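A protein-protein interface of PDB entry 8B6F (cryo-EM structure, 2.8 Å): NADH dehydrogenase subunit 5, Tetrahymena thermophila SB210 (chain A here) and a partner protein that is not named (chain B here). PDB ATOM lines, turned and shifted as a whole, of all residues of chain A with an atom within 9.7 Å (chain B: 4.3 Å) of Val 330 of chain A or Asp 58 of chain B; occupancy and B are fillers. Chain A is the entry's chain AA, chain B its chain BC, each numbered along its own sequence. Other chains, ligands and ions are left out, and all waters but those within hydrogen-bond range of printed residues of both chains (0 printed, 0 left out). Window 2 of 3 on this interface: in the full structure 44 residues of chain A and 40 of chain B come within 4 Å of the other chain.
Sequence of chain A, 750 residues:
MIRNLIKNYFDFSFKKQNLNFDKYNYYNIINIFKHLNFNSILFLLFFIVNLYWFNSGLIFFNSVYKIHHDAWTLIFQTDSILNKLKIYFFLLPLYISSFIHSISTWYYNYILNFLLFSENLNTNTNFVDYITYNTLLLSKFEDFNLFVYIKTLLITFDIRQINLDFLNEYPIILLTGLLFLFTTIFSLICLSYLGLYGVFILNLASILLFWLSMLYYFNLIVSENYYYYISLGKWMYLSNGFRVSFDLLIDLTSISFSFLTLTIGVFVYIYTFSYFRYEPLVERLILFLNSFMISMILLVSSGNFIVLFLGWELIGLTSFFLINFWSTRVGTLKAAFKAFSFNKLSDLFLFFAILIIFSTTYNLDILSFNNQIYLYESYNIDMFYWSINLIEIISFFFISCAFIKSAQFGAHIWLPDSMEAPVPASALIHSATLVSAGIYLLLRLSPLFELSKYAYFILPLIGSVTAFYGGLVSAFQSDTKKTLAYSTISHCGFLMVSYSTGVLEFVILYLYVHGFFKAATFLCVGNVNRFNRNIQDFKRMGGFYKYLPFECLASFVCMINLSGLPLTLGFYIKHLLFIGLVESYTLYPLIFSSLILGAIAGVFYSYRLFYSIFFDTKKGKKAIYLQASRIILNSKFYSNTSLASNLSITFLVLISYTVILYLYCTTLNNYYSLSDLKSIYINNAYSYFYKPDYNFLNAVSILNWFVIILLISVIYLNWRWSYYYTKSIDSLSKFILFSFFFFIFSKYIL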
ATOM      1  N   ILE A 323      10.752  -0.364 -20.968  1.00  0.00           N
ATOM      2  CA  ILE A 323      11.814   0.590 -21.273  1.00  0.00           C
ATOM      3  C   ILE A 323      12.461   1.088 -19.990  1.00  0.00           C
ATOM      4  O   ILE A 323      13.686   1.233 -19.908  1.00  0.00           O
ATOM      5  CB  ILE A 323      11.265   1.752 -22.123  1.00  0.00           C
ATOM      6  CG1 ILE A 323      10.751   1.229 -23.466  1.00  0.00           C
ATOM      7  CG2 ILE A 323      12.341   2.807 -22.350  1.00  0.00           C
ATOM      8  CD1 ILE A 323       9.900   2.222 -24.223  1.00  0.00           C
ATOM      9  N   ASN A 324      11.651   1.355 -18.968  1.00  0.00           N
ATOM     10  CA  ASN A 324      12.135   1.853 -17.691  1.00  0.00           C
ATOM     11  C   ASN A 324      12.518   0.730 -16.736  1.00  0.00           C
ATOM     12  O   ASN A 324      12.567   0.952 -15.522  1.00  0.00           O
ATOM     13  CB  ASN A 324      11.074   2.747 -17.047  1.00  0.00           C
ATOM     14  CG  ASN A 324      11.638   3.627 -15.956  1.00  0.00           C
ATOM     15  OD1 ASN A 324      12.830   3.924 -15.936  1.00  0.00           O
ATOM     16  ND2 ASN A 324      10.782   4.048 -15.036  1.00  0.00           N
ATOM     17  N   PHE A 325      12.781  -0.472 -17.255  1.00  0.00           N
ATOM     18  CA  PHE A 325      13.161  -1.582 -16.388  1.00  0.00           C
ATOM     19  C   PHE A 325      14.305  -1.208 -15.454  1.00  0.00           C
ATOM     20  O   PHE A 325      14.273  -1.533 -14.262  1.00  0.00           O
ATOM     21  CB  PHE A 325      13.541  -2.799 -17.231  1.00  0.00           C
ATOM     22  CG  PHE A 325      13.844  -4.017 -16.417  1.00  0.00           C
ATOM     23  CD1 PHE A 325      12.820  -4.836 -15.974  1.00  0.00           C
ATOM     24  CD2 PHE A 325      15.147  -4.343 -16.091  1.00  0.00           C
ATOM     25  CE1 PHE A 325      13.090  -5.956 -15.218  1.00  0.00           C
ATOM     26  CE2 PHE A 325      15.424  -5.463 -15.336  1.00  0.00           C
ATOM     27  CZ  PHE A 325      14.396  -6.271 -14.900  1.00  0.00           C
ATOM     28  N   TRP A 326      15.327  -0.525 -15.973  1.00  0.00           N
ATOM     29  CA  TRP A 326      16.435  -0.055 -15.141  1.00  0.00           C
ATOM     30  C   TRP A 326      15.976   1.189 -14.378  1.00  0.00           C
ATOM     31  O   TRP A 326      16.394   2.319 -14.636  1.00  0.00           O
ATOM     32  CB  TRP A 326      17.665   0.223 -15.995  1.00  0.00           C
ATOM     33  CG  TRP A 326      18.148  -0.974 -16.760  1.00  0.00           C
ATOM     34  CD1 TRP A 326      18.120  -1.146 -18.113  1.00  0.00           C
ATOM     35  CD2 TRP A 326      18.724  -2.169 -16.218  1.00  0.00           C
ATOM     36  NE1 TRP A 326      18.645  -2.370 -18.448  1.00  0.00           N
ATOM     37  CE2 TRP A 326      19.024  -3.018 -17.302  1.00  0.00           C
ATOM     38  CE3 TRP A 326      19.017  -2.603 -14.921  1.00  0.00           C
ATOM     39  CZ2 TRP A 326      19.601  -4.272 -17.129  1.00  0.00           C
ATOM     40  CZ3 TRP A 326      19.591  -3.849 -14.751  1.00  0.00           C
ATOM     41  CH2 TRP A 326      19.879  -4.669 -15.849  1.00  0.00           C
ATOM     42  N   SER A 327      15.093   0.953 -13.407  1.00  0.00           N
ATOM     43  CA  SER A 327      14.455   2.055 -12.692  1.00  0.00           C
ATOM     44  C   SER A 327      15.448   2.866 -11.868  1.00  0.00           C
ATOM     45  O   SER A 327      15.210   4.050 -11.611  1.00  0.00           O
ATOM     46  CB  SER A 327      13.345   1.512 -11.796  1.00  0.00           C
ATOM     47  OG  SER A 327      13.806   0.423 -11.015  1.00  0.00           O
ATOM     48  N   THR A 328      16.554   2.257 -11.436  1.00  0.00           N
ATOM     49  CA  THR A 328      17.513   2.984 -10.611  1.00  0.00           C
ATOM     50  C   THR A 328      18.117   4.155 -11.371  1.00  0.00           C
ATOM     51  O   THR A 328      18.365   5.218 -10.792  1.00  0.00           O
ATOM     52  CB  THR A 328      18.620   2.051 -10.131  1.00  0.00           C
ATOM     53  OG1 THR A 328      19.245   1.440 -11.261  1.00  0.00           O
ATOM     54  CG2 THR A 328      18.057   0.974  -9.221  1.00  0.00           C
ATOM     55  N   ARG A 329      18.368   3.979 -12.664  1.00  0.00           N
ATOM     56  CA  ARG A 329      18.941   5.041 -13.475  1.00  0.00           C
ATOM     57  C   ARG A 329      17.860   6.007 -13.934  1.00  0.00           C
ATOM     58  O   ARG A 329      16.780   5.597 -14.366  1.00  0.00           O
ATOM     59  CB  ARG A 329      19.654   4.457 -14.695  1.00  0.00           C
ATOM     60  CG  ARG A 329      20.995   3.819 -14.393  1.00  0.00           C
ATOM     61  CD  ARG A 329      21.575   3.146 -15.628  1.00  0.00           C
ATOM     62  NE  ARG A 329      21.421   3.967 -16.824  1.00  0.00           N
ATOM     63  CZ  ARG A 329      22.208   4.985 -17.146  1.00  0.00           C
ATOM     64  NH1 ARG A 329      23.220   5.349 -16.376  1.00  0.00           N
ATOM     65  NH2 ARG A 329      21.974   5.654 -18.271  1.00  0.00           N
ATOM     66  N   VAL A 330      18.161   7.302 -13.835  1.00  0.00           N
ATOM     67  CA  VAL A 330      17.260   8.322 -14.355  1.00  0.00           C
ATOM     68  C   VAL A 330      17.484   8.587 -15.839  1.00  0.00           C
ATOM     69  O   VAL A 330      16.612   9.181 -16.488  1.00  0.00           O
ATOM     70  CB  VAL A 330      17.393   9.639 -13.572  1.00  0.00           C
ATOM     71  CG1 VAL A 330      16.870   9.463 -12.158  1.00  0.00           C
ATOM     72  CG2 VAL A 330      18.838  10.131 -13.565  1.00  0.00           C
ATOM     73  N   GLY A 331      18.625   8.176 -16.392  1.00  0.00           N
ATOM     74  CA  GLY A 331      18.806   8.275 -17.828  1.00  0.00           C
ATOM     75  C   GLY A 331      17.817   7.409 -18.582  1.00  0.00           C
ATOM     76  O   GLY A 331      17.281   7.815 -19.615  1.00  0.00           O
ATOM     77  N   THR A 332      17.568   6.199 -18.078  1.00  0.00           N
ATOM     78  CA  THR A 332      16.535   5.352 -18.661  1.00  0.00           C
ATOM     79  C   THR A 332      15.155   5.979 -18.518  1.00  0.00           C
ATOM     80  O   THR A 332      14.307   5.819 -19.400  1.00  0.00           O
ATOM     81  CB  THR A 332      16.552   3.974 -17.999  1.00  0.00           C
ATOM     82  OG1 THR A 332      17.866   3.410 -18.096  1.00  0.00           O
ATOM     83  CG2 THR A 332      15.554   3.043 -18.668  1.00  0.00           C
ATOM     84  N   LEU A 333      14.910   6.683 -17.411  1.00  0.00           N
ATOM     85  CA  LEU A 333      13.605   7.295 -17.201  1.00  0.00           C
ATOM     86  C   LEU A 333      13.303   8.350 -18.254  1.00  0.00           C
ATOM     87  O   LEU A 333      12.133   8.578 -18.585  1.00  0.00           O
ATOM     88  CB  LEU A 333      13.533   7.906 -15.802  1.00  0.00           C
ATOM     89  CG  LEU A 333      12.224   8.607 -15.432  1.00  0.00           C
ATOM     90  CD1 LEU A 333      11.039   7.673 -15.586  1.00  0.00           C
ATOM     91  CD2 LEU A 333      12.301   9.140 -14.016  1.00  0.00           C
ATOM     92  N   LYS A 334      14.331   9.009 -18.788  1.00  0.00           N
ATOM     93  CA  LYS A 334      14.099  10.011 -19.820  1.00  0.00           C
ATOM     94  C   LYS A 334      13.577   9.367 -21.097  1.00  0.00           C
ATOM     95  O   LYS A 334      12.624   9.864 -21.710  1.00  0.00           O
ATOM     96  CB  LYS A 334      15.383  10.794 -20.093  1.00  0.00           C
ATOM     97  CG  LYS A 334      15.874  11.598 -18.902  1.00  0.00           C
ATOM     98  CD  LYS A 334      16.918  12.628 -19.302  1.00  0.00           C
ATOM     99  CE  LYS A 334      18.144  11.983 -19.920  1.00  0.00           C
ATOM    100  NZ  LYS A 334      19.217  12.983 -20.176  1.00  0.00           N
ATOM    101  N   ALA A 335      14.192   8.263 -21.523  1.00  0.00           N
ATOM    102  CA  ALA A 335      13.680   7.548 -22.687  1.00  0.00           C
ATOM    103  C   ALA A 335      12.284   7.003 -22.423  1.00  0.00           C
ATOM    104  O   ALA A 335      11.410   7.057 -23.295  1.00  0.00           O
ATOM    105  CB  ALA A 335      14.629   6.415 -23.069  1.00  0.00           C
ATOM    106  N   ALA A 336      12.059   6.463 -21.225  1.00  0.00           N
ATOM    107  CA  ALA A 336      10.737   5.954 -20.883  1.00  0.00           C
ATOM    108  C   ALA A 336       9.696   7.062 -20.939  1.00  0.00           C
ATOM    109  O   ALA A 336       8.577   6.853 -21.420  1.00  0.00           O
ATOM    110  CB  ALA A 336      10.767   5.312 -19.499  1.00  0.00           C
ATOM    111  N   PHE A 337      10.053   8.253 -20.454  1.00  0.00           N
ATOM    112  CA  PHE A 337       9.120   9.373 -20.457  1.00  0.00           C
ATOM    113  C   PHE A 337       8.872   9.887 -21.868  1.00  0.00           C
ATOM    114  O   PHE A 337       7.758  10.320 -22.182  1.00  0.00           O
ATOM    115  CB  PHE A 337       9.653  10.492 -19.561  1.00  0.00           C
ATOM    116  CG  PHE A 337       8.594  11.440 -19.076  1.00  0.00           C
ATOM    117  CD1 PHE A 337       7.540  10.983 -18.301  1.00  0.00           C
ATOM    118  CD2 PHE A 337       8.668  12.789 -19.369  1.00  0.00           C
ATOM    119  CE1 PHE A 337       6.569  11.853 -17.847  1.00  0.00           C
ATOM    120  CE2 PHE A 337       7.701  13.663 -18.918  1.00  0.00           C
ATOM    121  CZ  PHE A 337       6.650  13.193 -18.156  1.00  0.00           C
ATOM    122  N   LYS A 338       9.892   9.857 -22.726  1.00  0.00           N
ATOM    123  CA  LYS A 338       9.686  10.194 -24.129  1.00  0.00           C
ATOM    124  C   LYS A 338       8.664   9.261 -24.764  1.00  0.00           C
ATOM    125  O   LYS A 338       7.712   9.709 -25.413  1.00  0.00           O
ATOM    126  CB  LYS A 338      11.022  10.116 -24.864  1.00  0.00           C
ATOM    127  CG  LYS A 338      11.038  10.729 -26.243  1.00  0.00           C
ATOM    128  CD  LYS A 338      12.437  10.615 -26.815  1.00  0.00           C
ATOM    129  CE  LYS A 338      12.648  11.543 -27.984  1.00  0.00           C
ATOM    130  NZ  LYS A 338      14.104  11.675 -28.275  1.00  0.00           N
ATOM    131  N   GLU A 420      16.954   1.289 -24.793  1.00  0.00           N
ATOM    132  CA  GLU A 420      17.489   1.129 -23.448  1.00  0.00           C
ATOM    133  C   GLU A 420      16.929  -0.108 -22.756  1.00  0.00           C
ATOM    134  O   GLU A 420      17.518  -0.578 -21.777  1.00  0.00           O
ATOM    135  CB  GLU A 420      17.181   2.376 -22.616  1.00  0.00           C
ATOM    136  CG  GLU A 420      17.926   2.449 -21.294  1.00  0.00           C
ATOM    137  CD  GLU A 420      19.422   2.595 -21.475  1.00  0.00           C
ATOM    138  OE1 GLU A 420      19.863   2.844 -22.616  1.00  0.00           O
ATOM    139  OE2 GLU A 420      20.159   2.462 -20.475  1.00  0.00           O
ATOM    140  N   MET B  56      16.193  16.217 -14.457  1.00  0.00           N
ATOM    141  CA  MET B  56      15.738  14.923 -13.951  1.00  0.00           C
ATOM    142  C   MET B  56      16.458  14.691 -12.631  1.00  0.00           C
ATOM    143  O   MET B  56      17.566  14.159 -12.583  1.00  0.00           O
ATOM    144  CB  MET B  56      16.015  13.814 -14.957  1.00  0.00           C
ATOM    145  CG  MET B  56      15.340  12.495 -14.621  1.00  0.00           C
ATOM    146  SD  MET B  56      13.538  12.577 -14.675  1.00  0.00           S
ATOM    147  CE  MET B  56      13.248  12.718 -16.435  1.00  0.00           C
ATOM    148  N   TYR B  57      15.817  15.107 -11.542  1.00  0.00           N
ATOM    149  CA  TYR B  57      16.479  15.121 -10.245  1.00  0.00           C
ATOM    150  C   TYR B  57      16.838  13.710  -9.803  1.00  0.00           C
ATOM    151  O   TYR B  57      16.059  12.768  -9.967  1.00  0.00           O
ATOM    152  CB  TYR B  57      15.578  15.783  -9.202  1.00  0.00           C
ATOM    153  CG  TYR B  57      15.209  17.207  -9.546  1.00  0.00           C
ATOM    154  CD1 TYR B  57      16.087  18.251  -9.299  1.00  0.00           C
ATOM    155  CD2 TYR B  57      13.979  17.505 -10.112  1.00  0.00           C
ATOM    156  CE1 TYR B  57      15.754  19.552  -9.613  1.00  0.00           C
ATOM    157  CE2 TYR B  57      13.635  18.802 -10.428  1.00  0.00           C
ATOM    158  CZ  TYR B  57      14.527  19.822 -10.175  1.00  0.00           C
ATOM    159  OH  TYR B  57      14.190  21.117 -10.488  1.00  0.00           O
ATOM    160  N   ASP B  58      18.037  13.569  -9.243  1.00  0.00           N
ATOM    161  CA  ASP B  58      18.492  12.297  -8.708  1.00  0.00           C
ATOM    162  C   ASP B  58      19.513  12.571  -7.617  1.00  0.00           C
ATOM    163  O   ASP B  58      20.116  13.645  -7.560  1.00  0.00           O
ATOM    164  CB  ASP B  58      19.096  11.410  -9.801  1.00  0.00           C
ATOM    165  CG  ASP B  58      19.346   9.994  -9.328  1.00  0.00           C
ATOM    166  OD1 ASP B  58      18.965   9.676  -8.185  1.00  0.00           O
ATOM    167  OD2 ASP B  58      19.921   9.199 -10.099  1.00  0.00           O
ATOM    168  N   GLN B  59      19.698  11.586  -6.744  1.00  0.00           N
ATOM    169  CA  GLN B  59      20.647  11.693  -5.646  1.00  0.00           C
ATOM    170  C   GLN B  59      22.007  11.096  -5.977  1.00  0.00           C
ATOM    171  O   GLN B  59      22.917  11.177  -5.147  1.00  0.00           O
ATOM    172  CB  GLN B  59      20.078  11.016  -4.396  1.00  0.00           C
ATOM    173  CG  GLN B  59      18.748  11.596  -3.949  1.00  0.00           C
ATOM    174  CD  GLN B  59      18.208  10.921  -2.712  1.00  0.00           C
ATOM    175  OE1 GLN B  59      18.887  10.110  -2.086  1.00  0.00           O
ATOM    176  NE2 GLN B  59      16.973  11.251  -2.351  1.00  0.00           N
ATOM    177  N   VAL B  60      22.168  10.502  -7.157  1.00  0.00           N
ATOM    178  CA  VAL B  60      23.435   9.891  -7.544  1.00  0.00           C
ATOM    179  C   VAL B  60      23.903  10.480  -8.867  1.00  0.00           C
ATOM    180  O   VAL B  60      25.010  11.020  -8.963  1.00  0.00           O
ATOM    181  CB  VAL B  60      23.301   8.359  -7.636  1.00  0.00           C
ATOM    182  CG1 VAL B  60      24.604   7.728  -8.093  1.00  0.00           C
ATOM    183  CG2 VAL B  60      22.879   7.787  -6.297  1.00  0.00           C
ATOM    184  N   TYR B  61      23.063  10.384  -9.896  1.00  0.00           N
ATOM    185  CA  TYR B  61      23.397  10.836 -11.247  1.00  0.00           C
ATOM    186  C   TYR B  61      22.268  11.703 -11.786  1.00  0.00           C
ATOM    187  O   TYR B  61      21.504  11.279 -12.660  1.00  0.00           O
ATOM    188  CB  TYR B  61      23.650   9.645 -12.172  1.00  0.00           C
ATOM    189  CG  TYR B  61      24.900   8.854 -11.856  1.00  0.00           C
ATOM    190  CD1 TYR B  61      26.074   9.490 -11.471  1.00  0.00           C
ATOM    191  CD2 TYR B  61      24.905   7.470 -11.945  1.00  0.00           C
ATOM    192  CE1 TYR B  61      27.215   8.770 -11.184  1.00  0.00           C
ATOM    193  CE2 TYR B  61      26.040   6.741 -11.661  1.00  0.00           C
ATOM    194  CZ  TYR B  61      27.192   7.396 -11.280  1.00  0.00           C
ATOM    195  OH  TYR B  61      28.324   6.669 -10.997  1.00  0.00           O
ATOM    196  N   PRO B  62      22.132  12.929 -11.283  1.00  0.00           N
ATOM    197  CA  PRO B  62      21.138  13.841 -11.858  1.00  0.00           C
ATOM    198  C   PRO B  62      21.465  14.157 -13.309  1.00  0.00           C
ATOM    199  O   PRO B  62      22.629  14.220 -13.707  1.00  0.00           O
ATOM    200  CB  PRO B  62      21.241  15.087 -10.970  1.00  0.00           C
ATOM    201  CG  PRO B  62      22.595  15.018 -10.374  1.00  0.00           C
ATOM    202  CD  PRO B  62      22.907  13.563 -10.206  1.00  0.00           C
ATOM    203  N   GLU B  63      20.417  14.357 -14.103  1.00  0.00           N
ATOM    204  CA  GLU B  63      20.569  14.564 -15.534  1.00  0.00           C
ATOM    205  C   GLU B  63      19.603  15.638 -16.007  1.00  0.00           C
ATOM    206  O   GLU B  63      18.546  15.850 -15.411  1.00  0.00           O
ATOM    207  CB  GLU B  63      20.316  13.268 -16.314  1.00  0.00           C
ATOM    208  CG  GLU B  63      21.254  12.137 -15.936  1.00  0.00           C
ATOM    209  CD  GLU B  63      21.068  10.913 -16.804  1.00  0.00           C
ATOM    210  OE1 GLU B  63      20.408  11.028 -17.857  1.00  0.00           O
ATOM    211  OE2 GLU B  63      21.578   9.836 -16.434  1.00  0.00           O
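Of the 17 printed residues of chain A, 4 touch a printed residue of chain B. Hydrophobic or aromatic side chains of chain A within 4 Å of the printed part of chain B: Val 330 and Leu 333. Of the 8 printed residues of chain B, 4 touch a printed residue of chain A. Among the printed residues, 8 pairs touch across the chains.
Among the printed residues, pairs that only touch across the chains: Val 330 of chain A with Met 56 of chain B (3.7 Å), Val 330 of chain A with Asp 58 of chain B (3.7 Å), Val 330 of chain A with Tyr 61 of chain B (3.0 Å), Val 330 of chain A with Glu 63 of chain B (3.9 Å), Leu 333 of chain A with Met 56 of chain B (3.7 Å) and Lys 334 of chain A with Met 56 of chain B (3.8 Å).
N of Met 56 of chain B lies within hydrogen-bond range of O of Glu 63 of chain B (2.6 Å). The side-chain carboxylate (OD1) of Asp 58 of chain B lies close to the backbone NH (N) of Val 60 of chain B, 3.5 Å away. The side-chain carboxylate of Asp 58 of chain B lies within hydrogen-bond range of the backbone NH of Tyr 61 of chain B (3.4 Å).
The backbone NH of Gly 331 of chain A sits at hydrogen-bond distance from the side-chain carboxylate of Glu 63 of chain B, 3.4 Å away. The side-chain amino group (NZ) of Lys 334 of chain A lies within salt-bridge range of the side-chain carboxylate (OE1) of Glu 63 of chain B, 3.3 Å away.
Printed residues of chain B within 4 Å of Val 330 of chain A: Met 56 (3.7 Å), Asp 58 (3.7 Å), Tyr 61 (3.0 Å) and Glu 63 (3.9 Å). Of the printed residues of chain B, Leu 333 of chain A touches Met 56 (3.7 Å). Of the printed residues of chain A, Met 56 of chain B touches Val 330 (3.7 Å), Leu 333 (3.7 Å) and Lys 334 (3.8 Å). Of the printed residues of chain B, Lys 334 of chain A touches Met 56 (3.8 Å) and Glu 63 (3.2 Å). Of the printed residues of chain B, Gly 331 of chain A touches Glu 63 (3.2 Å). Of the printed residues of chain A, Tyr 61 of chain B touches Val 330 (3.0 Å). Ala 335 of chain A touches none of the printed residues of chain B. Asn 324 of chain A touches none of the printed residues of chain B.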
